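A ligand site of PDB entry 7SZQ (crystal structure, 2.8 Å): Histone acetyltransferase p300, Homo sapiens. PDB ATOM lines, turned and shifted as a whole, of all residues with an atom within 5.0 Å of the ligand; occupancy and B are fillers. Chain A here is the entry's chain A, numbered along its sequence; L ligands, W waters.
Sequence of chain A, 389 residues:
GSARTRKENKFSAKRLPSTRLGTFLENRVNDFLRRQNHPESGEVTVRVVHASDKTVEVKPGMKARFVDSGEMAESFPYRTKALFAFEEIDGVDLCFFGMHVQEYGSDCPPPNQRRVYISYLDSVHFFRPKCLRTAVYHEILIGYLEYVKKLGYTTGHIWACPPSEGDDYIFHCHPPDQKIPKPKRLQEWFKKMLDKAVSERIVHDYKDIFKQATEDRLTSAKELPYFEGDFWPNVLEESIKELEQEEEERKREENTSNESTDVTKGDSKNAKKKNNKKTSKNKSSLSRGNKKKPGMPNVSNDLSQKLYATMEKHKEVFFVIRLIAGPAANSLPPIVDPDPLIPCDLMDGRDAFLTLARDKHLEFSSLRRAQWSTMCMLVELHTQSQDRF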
ATOM      1  N   PHE A  97     -34.456 -19.285 -14.538  1.00  0.00           N
ATOM      2  CA  PHE A  97     -35.095 -20.581 -14.702  1.00  0.00           C
ATOM      3  C   PHE A  97     -36.130 -20.484 -15.809  1.00  0.00           C
ATOM      4  O   PHE A  97     -36.949 -19.559 -15.804  1.00  0.00           O
ATOM      5  CB  PHE A  97     -35.745 -21.000 -13.386  1.00  0.00           C
ATOM      6  CG  PHE A  97     -36.493 -22.303 -13.465  1.00  0.00           C
ATOM      7  CD1 PHE A  97     -35.865 -23.504 -13.201  1.00  0.00           C
ATOM      8  CD2 PHE A  97     -37.836 -22.336 -13.834  1.00  0.00           C
ATOM      9  CE1 PHE A  97     -36.571 -24.697 -13.280  1.00  0.00           C
ATOM     10  CE2 PHE A  97     -38.524 -23.539 -13.900  1.00  0.00           C
ATOM     11  CZ  PHE A  97     -37.892 -24.707 -13.631  1.00  0.00           C
ATOM     12  N   LEU A 121     -35.708 -28.263 -19.456  1.00  0.00           N
ATOM     13  CA  LEU A 121     -35.431 -27.476 -18.269  1.00  0.00           C
ATOM     14  C   LEU A 121     -34.066 -26.820 -18.407  1.00  0.00           C
ATOM     15  O   LEU A 121     -33.100 -27.441 -18.856  1.00  0.00           O
ATOM     16  CB  LEU A 121     -35.457 -28.322 -16.972  1.00  0.00           C
ATOM     17  CG  LEU A 121     -36.819 -28.825 -16.509  1.00  0.00           C
ATOM     18  CD1 LEU A 121     -36.687 -29.695 -15.303  1.00  0.00           C
ATOM     19  CD2 LEU A 121     -37.722 -27.659 -16.189  1.00  0.00           C
ATOM     20  N   ASP A 122     -33.985 -25.554 -18.017  1.00  0.00           N
ATOM     21  CA  ASP A 122     -32.737 -24.838 -18.101  1.00  0.00           C
ATOM     22  C   ASP A 122     -32.686 -23.846 -16.968  1.00  0.00           C
ATOM     23  O   ASP A 122     -33.721 -23.406 -16.461  1.00  0.00           O
ATOM     24  CB  ASP A 122     -32.580 -24.104 -19.440  1.00  0.00           C
ATOM     25  CG  ASP A 122     -31.124 -23.890 -19.823  1.00  0.00           C
ATOM     26  OD1 ASP A 122     -30.240 -24.248 -19.026  1.00  0.00           O
ATOM     27  OD2 ASP A 122     -30.876 -23.365 -20.929  1.00  0.00           O
ATOM     28  N   SER A 123     -31.470 -23.470 -16.589  1.00  0.00           N
ATOM     29  CA  SER A 123     -31.312 -22.440 -15.582  1.00  0.00           C
ATOM     30  C   SER A 123     -30.014 -21.690 -15.799  1.00  0.00           C
ATOM     31  O   SER A 123     -29.154 -22.094 -16.599  1.00  0.00           O
ATOM     32  CB  SER A 123     -31.303 -23.012 -14.170  1.00  0.00           C
ATOM     33  OG  SER A 123     -30.259 -23.968 -14.075  1.00  0.00           O
ATOM     34  N   TYR A 137     -35.544 -24.246  -7.138  1.00  0.00           N
ATOM     35  CA  TYR A 137     -35.894 -25.066  -8.302  1.00  0.00           C
ATOM     36  C   TYR A 137     -36.862 -26.171  -7.906  1.00  0.00           C
ATOM     37  O   TYR A 137     -37.777 -26.517  -8.660  1.00  0.00           O
ATOM     38  CB  TYR A 137     -34.653 -25.709  -8.932  1.00  0.00           C
ATOM     39  CG  TYR A 137     -33.631 -24.761  -9.494  1.00  0.00           C
ATOM     40  CD1 TYR A 137     -33.979 -23.470  -9.885  1.00  0.00           C
ATOM     41  CD2 TYR A 137     -32.324 -25.171  -9.681  1.00  0.00           C
ATOM     42  CE1 TYR A 137     -33.027 -22.613 -10.404  1.00  0.00           C
ATOM     43  CE2 TYR A 137     -31.374 -24.337 -10.207  1.00  0.00           C
ATOM     44  CZ  TYR A 137     -31.731 -23.066 -10.563  1.00  0.00           C
ATOM     45  OH  TYR A 137     -30.780 -22.232 -11.089  1.00  0.00           O
ATOM     46  N   LEU A 141     -40.729 -26.830  -9.327  1.00  0.00           N
ATOM     47  CA  LEU A 141     -41.075 -28.095  -9.973  1.00  0.00           C
ATOM     48  C   LEU A 141     -42.164 -28.829  -9.206  1.00  0.00           C
ATOM     49  O   LEU A 141     -43.130 -29.310  -9.809  1.00  0.00           O
ATOM     50  CB  LEU A 141     -39.818 -28.949 -10.108  1.00  0.00           C
ATOM     51  CG  LEU A 141     -38.913 -28.418 -11.193  1.00  0.00           C
ATOM     52  CD1 LEU A 141     -37.627 -29.251 -11.278  1.00  0.00           C
ATOM     53  CD2 LEU A 141     -39.691 -28.524 -12.460  1.00  0.00           C
ATOM     54  N   CYS A 161     -32.106 -35.756 -19.318  1.00  0.00           N
ATOM     55  CA  CYS A 161     -31.155 -35.687 -20.422  1.00  0.00           C
ATOM     56  C   CYS A 161     -30.250 -34.496 -20.202  1.00  0.00           C
ATOM     57  O   CYS A 161     -30.662 -33.337 -20.407  1.00  0.00           O
ATOM     58  CB  CYS A 161     -31.898 -35.554 -21.757  1.00  0.00           C
ATOM     59  SG  CYS A 161     -30.861 -35.666 -23.225  1.00  0.00           S
ATOM     60  N   PRO A 162     -29.005 -34.692 -19.770  1.00  0.00           N
ATOM     61  CA  PRO A 162     -28.068 -33.574 -19.701  1.00  0.00           C
ATOM     62  C   PRO A 162     -27.570 -33.206 -21.096  1.00  0.00           C
ATOM     63  O   PRO A 162     -27.296 -34.093 -21.911  1.00  0.00           O
ATOM     64  CB  PRO A 162     -26.939 -34.081 -18.797  1.00  0.00           C
ATOM     65  CG  PRO A 162     -27.145 -35.557 -18.675  1.00  0.00           C
ATOM     66  CD  PRO A 162     -28.465 -35.945 -19.252  1.00  0.00           C
ATOM     67  N   PRO A 163     -27.471 -31.914 -21.396  1.00  0.00           N
ATOM     68  CA  PRO A 163     -27.056 -31.492 -22.737  1.00  0.00           C
ATOM     69  C   PRO A 163     -25.586 -31.795 -23.028  1.00  0.00           C
ATOM     70  O   PRO A 163     -24.783 -32.075 -22.132  1.00  0.00           O
ATOM     71  CB  PRO A 163     -27.290 -29.979 -22.721  1.00  0.00           C
ATOM     72  CG  PRO A 163     -27.264 -29.606 -21.270  1.00  0.00           C
ATOM     73  CD  PRO A 163     -27.876 -30.774 -20.563  1.00  0.00           C
ATOM     74  N   SER A 164     -25.264 -31.742 -24.310  1.00  0.00           N
ATOM     75  CA  SER A 164     -23.876 -31.758 -24.754  1.00  0.00           C
ATOM     76  C   SER A 164     -23.248 -30.407 -24.453  1.00  0.00           C
ATOM     77  O   SER A 164     -23.914 -29.379 -24.506  1.00  0.00           O
ATOM     78  CB  SER A 164     -23.780 -32.029 -26.252  1.00  0.00           C
ATOM     79  OG  SER A 164     -24.463 -33.198 -26.645  1.00  0.00           O
ATOM     80  N   GLU A 165     -21.945 -30.429 -24.146  1.00  0.00           N
ATOM     81  CA  GLU A 165     -21.202 -29.176 -23.991  1.00  0.00           C
ATOM     82  C   GLU A 165     -21.491 -28.245 -25.164  1.00  0.00           C
ATOM     83  O   GLU A 165     -21.277 -28.605 -26.330  1.00  0.00           O
ATOM     84  CB  GLU A 165     -19.692 -29.471 -23.896  1.00  0.00           C
ATOM     85  CG  GLU A 165     -18.750 -28.249 -23.658  1.00  0.00           C
ATOM     86  CD  GLU A 165     -18.913 -27.529 -22.290  1.00  0.00           C
ATOM     87  OE1 GLU A 165     -19.577 -28.032 -21.355  1.00  0.00           O
ATOM     88  OE2 GLU A 165     -18.381 -26.397 -22.169  1.00  0.00           O
ATOM     89  N   GLY A 166     -22.027 -27.056 -24.862  1.00  0.00           N
ATOM     90  CA  GLY A 166     -22.324 -26.060 -25.862  1.00  0.00           C
ATOM     91  C   GLY A 166     -23.762 -26.050 -26.356  1.00  0.00           C
ATOM     92  O   GLY A 166     -24.205 -25.047 -26.941  1.00  0.00           O
ATOM     93  N   ASP A 167     -24.505 -27.127 -26.148  1.00  0.00           N
ATOM     94  CA  ASP A 167     -25.919 -27.168 -26.486  1.00  0.00           C
ATOM     95  C   ASP A 167     -26.680 -26.451 -25.372  1.00  0.00           C
ATOM     96  O   ASP A 167     -26.828 -26.983 -24.266  1.00  0.00           O
ATOM     97  CB  ASP A 167     -26.399 -28.602 -26.657  1.00  0.00           C
ATOM     98  CG  ASP A 167     -27.683 -28.714 -27.487  1.00  0.00           C
ATOM     99  OD1 ASP A 167     -27.871 -27.922 -28.434  1.00  0.00           O
ATOM    100  OD2 ASP A 167     -28.499 -29.612 -27.192  1.00  0.00           O
ATOM    101  N   ASP A 168     -27.152 -25.242 -25.655  1.00  0.00           N
ATOM    102  CA  ASP A 168     -28.004 -24.497 -24.743  1.00  0.00           C
ATOM    103  C   ASP A 168     -29.439 -24.919 -24.986  1.00  0.00           C
ATOM    104  O   ASP A 168     -29.889 -24.911 -26.141  1.00  0.00           O
ATOM    105  CB  ASP A 168     -27.867 -22.990 -24.945  1.00  0.00           C
ATOM    106  CG  ASP A 168     -26.495 -22.473 -24.607  1.00  0.00           C
ATOM    107  OD1 ASP A 168     -25.915 -22.975 -23.629  1.00  0.00           O
ATOM    108  OD2 ASP A 168     -25.992 -21.564 -25.288  1.00  0.00           O
ATOM    109  N   TYR A 169     -30.151 -25.265 -23.914  1.00  0.00           N
ATOM    110  CA  TYR A 169     -31.551 -25.646 -24.038  1.00  0.00           C
ATOM    111  C   TYR A 169     -32.458 -24.422 -24.146  1.00  0.00           C
ATOM    112  O   TYR A 169     -33.313 -24.361 -25.028  1.00  0.00           O
ATOM    113  CB  TYR A 169     -31.981 -26.530 -22.860  1.00  0.00           C
ATOM    114  CG  TYR A 169     -31.555 -27.979 -22.932  1.00  0.00           C
ATOM    115  CD1 TYR A 169     -30.983 -28.512 -24.073  1.00  0.00           C
ATOM    116  CD2 TYR A 169     -31.740 -28.829 -21.844  1.00  0.00           C
ATOM    117  CE1 TYR A 169     -30.603 -29.842 -24.131  1.00  0.00           C
ATOM    118  CE2 TYR A 169     -31.361 -30.169 -21.899  1.00  0.00           C
ATOM    119  CZ  TYR A 169     -30.800 -30.667 -23.038  1.00  0.00           C
ATOM    120  OH  TYR A 169     -30.418 -31.988 -23.099  1.00  0.00           O
ATOM    121  N   HIS A 174     -24.296 -20.151 -21.611  1.00  0.00           N
ATOM    122  CA  HIS A 174     -24.258 -20.338 -20.174  1.00  0.00           C
ATOM    123  C   HIS A 174     -22.910 -19.840 -19.637  1.00  0.00           C
ATOM    124  O   HIS A 174     -21.959 -19.631 -20.397  1.00  0.00           O
ATOM    125  CB  HIS A 174     -24.461 -21.818 -19.825  1.00  0.00           C
ATOM    126  CG  HIS A 174     -25.902 -22.256 -19.845  1.00  0.00           C
ATOM    127  ND1 HIS A 174     -26.556 -22.617 -21.009  1.00  0.00           N
ATOM    128  CD2 HIS A 174     -26.802 -22.422 -18.852  1.00  0.00           C
ATOM    129  CE1 HIS A 174     -27.795 -22.976 -20.727  1.00  0.00           C
ATOM    130  NE2 HIS A 174     -27.972 -22.866 -19.419  1.00  0.00           N
ATOM    131  N   PRO A 175     -22.814 -19.629 -18.326  1.00  0.00           N
ATOM    132  CA  PRO A 175     -21.536 -19.300 -17.757  1.00  0.00           C
ATOM    133  C   PRO A 175     -20.565 -20.441 -17.993  1.00  0.00           C
ATOM    134  O   PRO A 175     -20.920 -21.629 -17.883  1.00  0.00           O
ATOM    135  CB  PRO A 175     -21.837 -19.111 -16.267  1.00  0.00           C
ATOM    136  CG  PRO A 175     -23.304 -18.891 -16.204  1.00  0.00           C
ATOM    137  CD  PRO A 175     -23.857 -19.714 -17.289  1.00  0.00           C
ATOM    138  N   GLN A 178     -20.526 -22.933 -15.051  1.00  0.00           N
ATOM    139  CA  GLN A 178     -21.698 -23.705 -14.659  1.00  0.00           C
ATOM    140  C   GLN A 178     -21.525 -25.114 -15.193  1.00  0.00           C
ATOM    141  O   GLN A 178     -21.645 -25.359 -16.391  1.00  0.00           O
ATOM    142  CB  GLN A 178     -22.985 -23.077 -15.197  1.00  0.00           C
ATOM    143  CG  GLN A 178     -24.274 -23.654 -14.586  1.00  0.00           C
ATOM    144  CD  GLN A 178     -25.565 -22.962 -15.056  1.00  0.00           C
ATOM    145  OE1 GLN A 178     -25.560 -21.765 -15.306  1.00  0.00           O
ATOM    146  NE2 GLN A 178     -26.674 -23.707 -15.123  1.00  0.00           N
ATOM    147  N   LYS A 179     -21.208 -26.049 -14.294  1.00  0.00           N
ATOM    148  CA  LYS A 179     -21.000 -27.431 -14.719  1.00  0.00           C
ATOM    149  C   LYS A 179     -22.300 -28.001 -15.254  1.00  0.00           C
ATOM    150  O   LYS A 179     -23.381 -27.739 -14.731  1.00  0.00           O
ATOM    151  CB  LYS A 179     -20.485 -28.270 -13.531  1.00  0.00           C
ATOM    152  N   ILE A 180     -22.198 -28.778 -16.326  1.00  0.00           N
ATOM    153  CA  ILE A 180     -23.320 -29.620 -16.746  1.00  0.00           C
ATOM    154  C   ILE A 180     -23.318 -30.876 -15.895  1.00  0.00           C
ATOM    155  O   ILE A 180     -22.272 -31.533 -15.764  1.00  0.00           O
ATOM    156  CB  ILE A 180     -23.192 -29.953 -18.218  1.00  0.00           C
ATOM    157  CG1 ILE A 180     -23.327 -28.678 -19.049  1.00  0.00           C
ATOM    158  CG2 ILE A 180     -24.263 -30.976 -18.608  1.00  0.00           C
ATOM    159  CD1 ILE A 180     -22.986 -28.854 -20.508  1.00  0.00           C
ATOM    160  N   PRO A 181     -24.442 -31.250 -15.291  1.00  0.00           N
ATOM    161  CA  PRO A 181     -24.447 -32.438 -14.434  1.00  0.00           C
ATOM    162  C   PRO A 181     -24.311 -33.723 -15.239  1.00  0.00           C
ATOM    163  O   PRO A 181     -24.880 -33.874 -16.327  1.00  0.00           O
ATOM    164  CB  PRO A 181     -25.821 -32.369 -13.743  1.00  0.00           C
ATOM    165  CG  PRO A 181     -26.656 -31.542 -14.609  1.00  0.00           C
ATOM    166  CD  PRO A 181     -25.731 -30.547 -15.245  1.00  0.00           C
ATOM    167  N   ARG A 185     -25.933 -37.772 -11.536  1.00  0.00           N
ATOM    168  CA  ARG A 185     -26.169 -36.620 -10.669  1.00  0.00           C
ATOM    169  C   ARG A 185     -27.517 -36.000 -10.957  1.00  0.00           C
ATOM    170  O   ARG A 185     -28.260 -35.643 -10.036  1.00  0.00           O
ATOM    171  CB  ARG A 185     -25.064 -35.583 -10.829  1.00  0.00           C
ATOM    172  CG  ARG A 185     -25.177 -34.414  -9.868  1.00  0.00           C
ATOM    173  CD  ARG A 185     -23.823 -33.951  -9.304  1.00  0.00           C
ATOM    174  N   LEU A 186     -27.876 -35.897 -12.237  1.00  0.00           N
ATOM    175  CA  LEU A 186     -29.148 -35.304 -12.603  1.00  0.00           C
ATOM    176  C   LEU A 186     -30.297 -36.212 -12.192  1.00  0.00           C
ATOM    177  O   LEU A 186     -31.353 -35.746 -11.749  1.00  0.00           O
ATOM    178  CB  LEU A 186     -29.183 -35.023 -14.109  1.00  0.00           C
ATOM    179  CG  LEU A 186     -30.470 -34.464 -14.699  1.00  0.00           C
ATOM    180  CD1 LEU A 186     -30.856 -33.177 -13.996  1.00  0.00           C
ATOM    181  CD2 LEU A 186     -30.299 -34.208 -16.168  1.00  0.00           C
ATOM    182  N   TRP A 189     -30.696 -35.875  -8.471  1.00  0.00           N
ATOM    183  CA  TRP A 189     -31.295 -34.571  -8.179  1.00  0.00           C
ATOM    184  C   TRP A 189     -32.803 -34.610  -8.395  1.00  0.00           C
ATOM    185  O   TRP A 189     -33.570 -34.069  -7.576  1.00  0.00           O
ATOM    186  CB  TRP A 189     -30.617 -33.493  -9.035  1.00  0.00           C
ATOM    187  CG  TRP A 189     -30.988 -32.065  -8.761  1.00  0.00           C
ATOM    188  CD1 TRP A 189     -30.309 -31.177  -7.973  1.00  0.00           C
ATOM    189  CD2 TRP A 189     -32.081 -31.326  -9.339  1.00  0.00           C
ATOM    190  NE1 TRP A 189     -30.938 -29.936  -8.002  1.00  0.00           N
ATOM    191  CE2 TRP A 189     -32.030 -30.018  -8.832  1.00  0.00           C
ATOM    192  CE3 TRP A 189     -33.104 -31.656 -10.241  1.00  0.00           C
ATOM    193  CZ2 TRP A 189     -32.952 -29.039  -9.189  1.00  0.00           C
ATOM    194  CZ3 TRP A 189     -34.024 -30.690 -10.572  1.00  0.00           C
ATOM    195  CH2 TRP A 189     -33.940 -29.398 -10.062  1.00  0.00           C
HETATM  196  N1  LIG L   1     -30.518 -28.337 -16.072  1.00  0.00           N
HETATM  197  C1  LIG L   1     -30.398 -30.403 -17.453  1.00  0.00           C
HETATM  198  C2  LIG L   1     -30.063 -29.180 -18.314  1.00  0.00           C
HETATM  199  C3  LIG L   1     -30.005 -27.954 -17.379  1.00  0.00           C
HETATM  200  C4  LIG L   1     -28.567 -27.527 -17.393  1.00  0.00           C
HETATM  201  O1  LIG L   1     -27.775 -28.054 -16.649  1.00  0.00           O
HETATM  202  C5  LIG L   1     -28.445 -30.178 -11.672  1.00  0.00           C
HETATM  203  C6  LIG L   1     -28.012 -29.037 -12.364  1.00  0.00           C
HETATM  204  C7  LIG L   1     -28.943 -28.281 -13.069  1.00  0.00           C
HETATM  205  C8  LIG L   1     -30.280 -28.665 -13.063  1.00  0.00           C
HETATM  206  C9  LIG L   1     -30.709 -29.801 -12.387  1.00  0.00           C
HETATM  207  C10 LIG L   1     -29.794 -30.565 -11.681  1.00  0.00           C
HETATM  208  C11 LIG L   1     -31.302 -27.841 -13.774  1.00  0.00           C
HETATM  209  C12 LIG L   1     -31.505 -26.600 -12.909  1.00  0.00           C
HETATM  210  C13 LIG L   1     -32.997 -26.225 -13.045  1.00  0.00           C
HETATM  211  C14 LIG L   1     -33.757 -27.529 -13.305  1.00  0.00           C
HETATM  212  C15 LIG L   1     -32.693 -28.498 -13.856  1.00  0.00           C
HETATM  213  C16 LIG L   1     -30.746 -27.455 -15.114  1.00  0.00           C
HETATM  214  C17 LIG L   1     -30.713 -29.805 -16.087  1.00  0.00           C
HETATM  215  C18 LIG L   1     -26.882 -26.155 -18.496  1.00  0.00           C
HETATM  216  C19 LIG L   1     -25.915 -25.875 -17.517  1.00  0.00           C
HETATM  217  C20 LIG L   1     -24.632 -25.497 -17.950  1.00  0.00           C
HETATM  218  C21 LIG L   1     -24.339 -25.430 -19.339  1.00  0.00           C
HETATM  219  C22 LIG L   1     -24.777 -25.578 -21.606  1.00  0.00           C
HETATM  220  C23 LIG L   1     -25.351 -25.744 -20.252  1.00  0.00           C
HETATM  221  N2  LIG L   1     -28.202 -26.585 -18.254  1.00  0.00           N
HETATM  222  N3  LIG L   1     -23.185 -25.098 -20.097  1.00  0.00           N
HETATM  223  N4  LIG L   1     -23.520 -25.208 -21.498  1.00  0.00           N
HETATM  224  N5  LIG L   1     -26.561 -26.098 -19.803  1.00  0.00           N
HETATM  225  O2  LIG L   1     -30.504 -26.265 -15.315  1.00  0.00           O
HETATM  226 CL1  LIG L   1     -27.307 -31.171 -10.791  1.00  0.00          CL
HETATM  227  O   HOH W   1     -20.751 -24.386 -19.130  1.00  0.00           O
HETATM  228  O   HOH W   2     -28.585 -26.038 -21.838  1.00  0.00           O
HETATM  229  O   HOH W   3     -26.262 -26.990 -14.573  1.00  0.00           O
HETATM  230  O   HOH W   4     -22.892 -22.464 -23.379  1.00  0.00           O
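N2 of the ligand lies within hydrogen-bond range of OD1 of Asp 122, at 3.2 Å.
O2 of the ligand lies within hydrogen-bond range of OG of Ser 123, at 2.6 Å.
The backbone NH of Ser 123 lies within hydrogen-bond range of an oxygen (O2) of the ligand (3.2 Å).
A ring nitrogen (ND1) of His 174 lies within hydrogen-bond range of the side-chain carboxylate (OD1) of Asp 168 (2.7 Å).
The backbone carbonyl oxygen (O) of Ser 123 sits at hydrogen-bond distance from the side-chain amide nitrogen (NE2) of Gln 178 (3.3 Å).
A ring nitrogen (NE2) of His 174 is in hydrogen-bond range of the backbone carbonyl oxygen (O) of Ser 123.
The side-chain hydroxyl (OH) of Tyr 137 lies close to the side-chain hydroxyl (OG) of Ser 123 (3.5 Å).
O of Cys 161 lies within hydrogen-bond range of OH of Tyr 169 (3.0 Å).
NE2 of His 174 is in hydrogen-bond range of OD1 of Asp 122, 2.7 Å away.
Residues that only touch the ligand: Gln 178 (3.3 Å), Trp 189 (3.4 Å), Ile 180 (3.4 Å), His 174 (3.4 Å), Leu 121 (3.5 Å), Asp 168 (3.5 Å), Pro 181 (3.5 Å), Pro 163 (3.5 Å), Tyr 137 (3.5 Å), Asp 167 (3.6 Å), Leu 186 (3.6 Å), Phe 97 (3.9 Å), Tyr 169 (3.9 Å) and Arg 185 (3.99 Å).
Within 4 Å of the ligand: Phe 97, Leu 121, Asp 122, Ser 123, Tyr 137, Pro 163, Asp 167, Asp 168, Tyr 169, His 174, Gln 178, Ile 180, Pro 181, Arg 185, Leu 186 and Trp 189.
The nearest printed residue that does not touch the ligand is Lys 179 (4.1 Å).
Water W1 lies within hydrogen-bond range of N3 of the ligand (2.7 Å), O of Pro 175 (3.0 Å) and O of Gln 178 (3.0 Å).
Water W3 lies within hydrogen-bond range of an oxygen (O1) of the ligand, the backbone carbonyl oxygen of Lys 179 and the side-chain amide nitrogen of Gln 178.
Water W2 lies within hydrogen-bond range of N of Tyr 169 (2.7 Å), N5 of the ligand (2.9 Å) and O of Asp 167 (3.1 Å).
Water W4 lies within hydrogen-bond range of the side-chain carboxylate (OD1) of Asp 168 (3.1 Å), the backbone NH (N) of His 174 (3.2 Å) and a nitrogen (N4) of the ligand (3.4 Å).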
